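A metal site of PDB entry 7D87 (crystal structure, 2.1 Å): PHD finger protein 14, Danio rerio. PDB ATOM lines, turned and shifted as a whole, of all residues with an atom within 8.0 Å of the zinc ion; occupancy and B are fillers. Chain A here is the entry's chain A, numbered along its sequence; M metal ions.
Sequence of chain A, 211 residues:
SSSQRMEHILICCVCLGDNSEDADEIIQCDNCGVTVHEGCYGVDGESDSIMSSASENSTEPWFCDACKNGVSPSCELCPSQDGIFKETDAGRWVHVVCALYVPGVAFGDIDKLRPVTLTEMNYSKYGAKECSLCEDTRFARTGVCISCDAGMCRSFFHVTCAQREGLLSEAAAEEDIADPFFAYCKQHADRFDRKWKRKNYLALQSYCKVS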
ATOM      1  N   GLN A  28       5.102  30.907 -20.338  1.00  0.00           N
ATOM      2  CA  GLN A  28       6.060  31.619 -21.172  1.00  0.00           C
ATOM      3  C   GLN A  28       7.481  31.163 -20.867  1.00  0.00           C
ATOM      4  O   GLN A  28       7.866  31.084 -19.697  1.00  0.00           O
ATOM      5  CB  GLN A  28       5.974  33.130 -20.972  1.00  0.00           C
ATOM      6  CG  GLN A  28       6.968  33.878 -21.813  1.00  0.00           C
ATOM      7  CD  GLN A  28       6.607  35.347 -21.944  1.00  0.00           C
ATOM      8  OE1 GLN A  28       5.949  35.901 -21.064  1.00  0.00           O
ATOM      9  NE2 GLN A  28       7.024  35.966 -23.034  1.00  0.00           N
ATOM     10  N   CYS A  29       8.248  30.879 -21.919  1.00  0.00           N
ATOM     11  CA  CYS A  29       9.650  30.514 -21.745  1.00  0.00           C
ATOM     12  C   CYS A  29      10.463  31.752 -21.370  1.00  0.00           C
ATOM     13  O   CYS A  29      10.434  32.756 -22.075  1.00  0.00           O
ATOM     14  CB  CYS A  29      10.207  29.881 -23.019  1.00  0.00           C
ATOM     15  SG  CYS A  29      11.961  29.482 -22.899  1.00  0.00           S
ATOM     16  N   ASP A  30      11.195  31.659 -20.263  1.00  0.00           N
ATOM     17  CA  ASP A  30      11.898  32.829 -19.762  1.00  0.00           C
ATOM     18  C   ASP A  30      13.209  33.116 -20.480  1.00  0.00           C
ATOM     19  O   ASP A  30      13.918  34.031 -20.070  1.00  0.00           O
ATOM     20  CB  ASP A  30      12.157  32.687 -18.262  1.00  0.00           C
ATOM     21  CG  ASP A  30      10.887  32.822 -17.443  1.00  0.00           C
ATOM     22  OD1 ASP A  30      10.092  33.753 -17.704  1.00  0.00           O
ATOM     23  OD2 ASP A  30      10.670  31.981 -16.552  1.00  0.00           O
ATOM     24  N   ASN A  31      13.572  32.360 -21.516  1.00  0.00           N
ATOM     25  CA  ASN A  31      14.739  32.708 -22.307  1.00  0.00           C
ATOM     26  C   ASN A  31      14.394  33.145 -23.727  1.00  0.00           C
ATOM     27  O   ASN A  31      14.831  34.216 -24.158  1.00  0.00           O
ATOM     28  CB  ASN A  31      15.737  31.554 -22.359  1.00  0.00           C
ATOM     29  CG  ASN A  31      16.893  31.823 -23.301  1.00  0.00           C
ATOM     30  OD1 ASN A  31      17.697  32.730 -23.068  1.00  0.00           O
ATOM     31  ND2 ASN A  31      16.981  31.055 -24.380  1.00  0.00           N
ATOM     32  N   CYS A  32      13.621  32.344 -24.473  1.00  0.00           N
ATOM     33  CA  CYS A  32      13.272  32.699 -25.851  1.00  0.00           C
ATOM     34  C   CYS A  32      11.947  33.434 -25.959  1.00  0.00           C
ATOM     35  O   CYS A  32      11.721  34.124 -26.957  1.00  0.00           O
ATOM     36  CB  CYS A  32      13.212  31.443 -26.726  1.00  0.00           C
ATOM     37  SG  CYS A  32      11.830  30.385 -26.351  1.00  0.00           S
ATOM     38  N   GLY A  33      11.067  33.313 -24.965  1.00  0.00           N
ATOM     39  CA  GLY A  33       9.862  34.106 -24.905  1.00  0.00           C
ATOM     40  C   GLY A  33       8.592  33.458 -25.441  1.00  0.00           C
ATOM     41  O   GLY A  33       7.529  34.071 -25.353  1.00  0.00           O
ATOM     42  N   VAL A  34       8.681  32.239 -26.001  1.00  0.00           N
ATOM     43  CA  VAL A  34       7.491  31.639 -26.585  1.00  0.00           C
ATOM     44  C   VAL A  34       6.473  31.327 -25.492  1.00  0.00           C
ATOM     45  O   VAL A  34       6.835  31.059 -24.335  1.00  0.00           O
ATOM     46  CB  VAL A  34       7.826  30.369 -27.406  1.00  0.00           C
ATOM     47  CG1 VAL A  34       8.784  30.719 -28.535  1.00  0.00           C
ATOM     48  CG2 VAL A  34       8.406  29.284 -26.508  1.00  0.00           C
ATOM     49  N   THR A  35       5.200  31.374 -25.863  1.00  0.00           N
ATOM     50  CA  THR A  35       4.077  31.170 -24.959  1.00  0.00           C
ATOM     51  C   THR A  35       3.234  30.003 -25.457  1.00  0.00           C
ATOM     52  O   THR A  35       2.995  29.884 -26.662  1.00  0.00           O
ATOM     53  CB  THR A  35       3.221  32.441 -24.864  1.00  0.00           C
ATOM     54  OG1 THR A  35       2.908  32.890 -26.190  1.00  0.00           O
ATOM     55  CG2 THR A  35       3.976  33.567 -24.148  1.00  0.00           C
ATOM     56  N   TYR A  41       1.758  21.321 -24.723  1.00  0.00           N
ATOM     57  CA  TYR A  41       3.189  21.046 -24.740  1.00  0.00           C
ATOM     58  C   TYR A  41       3.588  19.898 -23.836  1.00  0.00           C
ATOM     59  O   TYR A  41       4.774  19.563 -23.775  1.00  0.00           O
ATOM     60  CB  TYR A  41       3.981  22.300 -24.332  1.00  0.00           C
ATOM     61  CG  TYR A  41       5.458  22.313 -24.685  1.00  0.00           C
ATOM     62  CD1 TYR A  41       5.884  22.355 -26.007  1.00  0.00           C
ATOM     63  CD2 TYR A  41       6.432  22.334 -23.689  1.00  0.00           C
ATOM     64  CE1 TYR A  41       7.237  22.398 -26.329  1.00  0.00           C
ATOM     65  CE2 TYR A  41       7.778  22.373 -24.005  1.00  0.00           C
ATOM     66  CZ  TYR A  41       8.175  22.407 -25.329  1.00  0.00           C
ATOM     67  OH  TYR A  41       9.516  22.454 -25.645  1.00  0.00           O
ATOM     68  N   TRP A  62      10.275  29.120 -16.009  1.00  0.00           N
ATOM     69  CA  TRP A  62      10.065  27.970 -16.870  1.00  0.00           C
ATOM     70  C   TRP A  62      10.815  28.176 -18.174  1.00  0.00           C
ATOM     71  O   TRP A  62      10.910  29.294 -18.679  1.00  0.00           O
ATOM     72  CB  TRP A  62       8.573  27.721 -17.139  1.00  0.00           C
ATOM     73  CG  TRP A  62       8.336  26.535 -18.028  1.00  0.00           C
ATOM     74  CD1 TRP A  62       8.307  25.225 -17.643  1.00  0.00           C
ATOM     75  CD2 TRP A  62       8.103  26.550 -19.437  1.00  0.00           C
ATOM     76  NE1 TRP A  62       8.066  24.423 -18.737  1.00  0.00           N
ATOM     77  CE2 TRP A  62       7.935  25.213 -19.844  1.00  0.00           C
ATOM     78  CE3 TRP A  62       8.002  27.566 -20.390  1.00  0.00           C
ATOM     79  CZ2 TRP A  62       7.688  24.849 -21.177  1.00  0.00           C
ATOM     80  CZ3 TRP A  62       7.754  27.215 -21.718  1.00  0.00           C
ATOM     81  CH2 TRP A  62       7.607  25.872 -22.094  1.00  0.00           C
ATOM     82  N   PHE A  63      11.344  27.080 -18.717  1.00  0.00           N
ATOM     83  CA  PHE A  63      12.094  27.087 -19.961  1.00  0.00           C
ATOM     84  C   PHE A  63      11.627  25.972 -20.868  1.00  0.00           C
ATOM     85  O   PHE A  63      11.455  24.830 -20.416  1.00  0.00           O
ATOM     86  CB  PHE A  63      13.589  26.946 -19.693  1.00  0.00           C
ATOM     87  CG  PHE A  63      14.146  28.030 -18.833  1.00  0.00           C
ATOM     88  CD1 PHE A  63      14.425  29.281 -19.378  1.00  0.00           C
ATOM     89  CD2 PHE A  63      14.366  27.826 -17.486  1.00  0.00           C
ATOM     90  CE1 PHE A  63      14.918  30.300 -18.581  1.00  0.00           C
ATOM     91  CE2 PHE A  63      14.859  28.844 -16.690  1.00  0.00           C
ATOM     92  CZ  PHE A  63      15.144  30.074 -17.240  1.00  0.00           C
ATOM     93  N   CYS A  64      11.425  26.285 -22.144  1.00  0.00           N
ATOM     94  CA  CYS A  64      11.058  25.278 -23.124  1.00  0.00           C
ATOM     95  C   CYS A  64      12.221  24.299 -23.341  1.00  0.00           C
ATOM     96  O   CYS A  64      13.327  24.489 -22.821  1.00  0.00           O
ATOM     97  CB  CYS A  64      10.636  25.935 -24.434  1.00  0.00           C
ATOM     98  SG  CYS A  64      12.019  26.549 -25.431  1.00  0.00           S
ATOM     99  N   ASP A  65      11.964  23.239 -24.115  1.00  0.00           N
ATOM    100  CA  ASP A  65      12.971  22.186 -24.268  1.00  0.00           C
ATOM    101  C   ASP A  65      14.155  22.624 -25.116  1.00  0.00           C
ATOM    102  O   ASP A  65      15.291  22.182 -24.878  1.00  0.00           O
ATOM    103  CB  ASP A  65      12.345  20.920 -24.875  1.00  0.00           C
ATOM    104  CG  ASP A  65      11.360  20.231 -23.924  1.00  0.00           C
ATOM    105  OD1 ASP A  65      11.205  20.672 -22.765  1.00  0.00           O
ATOM    106  OD2 ASP A  65      10.727  19.231 -24.349  1.00  0.00           O
ATOM    107  N   ALA A  66      13.931  23.472 -26.135  1.00  0.00           N
ATOM    108  CA  ALA A  66      15.043  23.938 -26.949  1.00  0.00           C
ATOM    109  C   ALA A  66      16.018  24.767 -26.118  1.00  0.00           C
ATOM    110  O   ALA A  66      17.233  24.556 -26.187  1.00  0.00           O
ATOM    111  CB  ALA A  66      14.519  24.764 -28.126  1.00  0.00           C
ATOM    112  N   CYS A  67      15.488  25.671 -25.294  1.00  0.00           N
ATOM    113  CA  CYS A  67      16.354  26.499 -24.465  1.00  0.00           C
ATOM    114  C   CYS A  67      17.048  25.691 -23.383  1.00  0.00           C
ATOM    115  O   CYS A  67      18.218  25.943 -23.076  1.00  0.00           O
ATOM    116  CB  CYS A  67      15.536  27.638 -23.849  1.00  0.00           C
ATOM    117  SG  CYS A  67      14.985  28.815 -25.096  1.00  0.00           S
ATOM    118  N   LYS A  68      16.357  24.698 -22.802  1.00  0.00           N
ATOM    119  CA  LYS A  68      17.027  23.792 -21.862  1.00  0.00           C
ATOM    120  C   LYS A  68      18.295  23.208 -22.470  1.00  0.00           C
ATOM    121  O   LYS A  68      19.266  22.954 -21.756  1.00  0.00           O
ATOM    122  CB  LYS A  68      16.093  22.657 -21.444  1.00  0.00           C
ATOM    123  CG  LYS A  68      15.194  22.942 -20.267  1.00  0.00           C
ATOM    124  CD  LYS A  68      14.392  21.693 -19.914  1.00  0.00           C
ATOM    125  CE  LYS A  68      13.644  21.832 -18.598  1.00  0.00           C
ATOM    126  NZ  LYS A  68      12.563  22.836 -18.682  1.00  0.00           N
ATOM    127  N   VAL A  71      19.777  25.581 -27.676  1.00  0.00           N
ATOM    128  CA  VAL A  71      19.716  25.721 -29.125  1.00  0.00           C
ATOM    129  C   VAL A  71      18.514  26.560 -29.517  1.00  0.00           C
ATOM    130  O   VAL A  71      17.506  26.617 -28.799  1.00  0.00           O
ATOM    131  CB  VAL A  71      19.671  24.351 -29.839  1.00  0.00           C
ATOM    132  CG1 VAL A  71      20.898  23.514 -29.466  1.00  0.00           C
ATOM    133  CG2 VAL A  71      18.383  23.607 -29.514  1.00  0.00           C
ATOM    134  N   PRO A  73      16.625  26.018 -32.626  1.00  0.00           N
ATOM    135  CA  PRO A  73      16.757  25.036 -33.696  1.00  0.00           C
ATOM    136  C   PRO A  73      15.945  25.422 -34.936  1.00  0.00           C
ATOM    137  O   PRO A  73      15.171  26.379 -34.948  1.00  0.00           O
ATOM    138  CB  PRO A  73      16.203  23.769 -33.051  1.00  0.00           C
ATOM    139  CG  PRO A  73      15.131  24.287 -32.137  1.00  0.00           C
ATOM    140  CD  PRO A  73      15.652  25.606 -31.600  1.00  0.00           C
ATOM    141  N   GLY A  83       8.094  29.810 -32.961  1.00  0.00           N
ATOM    142  CA  GLY A  83       7.273  28.781 -32.358  1.00  0.00           C
ATOM    143  C   GLY A  83       8.058  27.920 -31.392  1.00  0.00           C
ATOM    144  O   GLY A  83       9.207  28.189 -31.039  1.00  0.00           O
ATOM    145  N   ILE A  84       7.423  26.837 -30.948  1.00  0.00           N
ATOM    146  CA  ILE A  84       7.969  26.008 -29.897  1.00  0.00           C
ATOM    147  C   ILE A  84       8.229  24.604 -30.435  1.00  0.00           C
ATOM    148  O   ILE A  84       7.496  24.108 -31.297  1.00  0.00           O
ATOM    149  CB  ILE A  84       7.035  26.018 -28.670  1.00  0.00           C
ATOM    150  CG1 ILE A  84       7.799  25.614 -27.411  1.00  0.00           C
ATOM    151  CG2 ILE A  84       5.773  25.201 -28.891  1.00  0.00           C
ATOM    152  CD1 ILE A  84       7.066  25.931 -26.124  1.00  0.00           C
ATOM    153  N   PHE A  85       9.320  23.984 -29.950  1.00  0.00           N
ATOM    154  CA  PHE A  85       9.916  22.793 -30.536  1.00  0.00           C
ATOM    155  C   PHE A  85       9.972  21.641 -29.546  1.00  0.00           C
ATOM    156  O   PHE A  85       9.962  21.834 -28.332  1.00  0.00           O
ATOM    157  CB  PHE A  85      11.353  23.066 -31.014  1.00  0.00           C
ATOM    158  CG  PHE A  85      11.455  24.019 -32.188  1.00  0.00           C
ATOM    159  CD1 PHE A  85      11.431  25.388 -31.999  1.00  0.00           C
ATOM    160  CD2 PHE A  85      11.619  23.530 -33.477  1.00  0.00           C
ATOM    161  CE1 PHE A  85      11.548  26.267 -33.079  1.00  0.00           C
ATOM    162  CE2 PHE A  85      11.732  24.391 -34.570  1.00  0.00           C
ATOM    163  CZ  PHE A  85      11.701  25.772 -34.354  1.00  0.00           C
HETATM  164 ZN    ZN M   1      12.607  28.804 -24.994  1.00  0.00          ZN
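The side-chain sulfur (SG) of Cys 32 lies close to the backbone NH (N) of Val 34 (3.7 Å). The backbone NH (N) of Cys 29 lies within hydrogen-bond range of the backbone carbonyl oxygen (O) of Val 34 (2.8 Å). SG of Cys 29 lies close to N of Asn 31 (3.6 Å). The side-chain sulfur (SG) of Cys 64 lies close to the backbone NH (N) of Ala 66, at 3.7 Å. The side-chain amide nitrogen of Asn 31 sits close to the side-chain sulfur of Cys 67.
The zinc ion is bound by the side-chain sulfur of Cys 32 (2.2 Å), the side-chain sulfur of Cys 29 (2.3 Å), the side-chain sulfur of Cys 64 (2.4 Å) and the side-chain sulfur of Cys 67 (2.4 Å).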
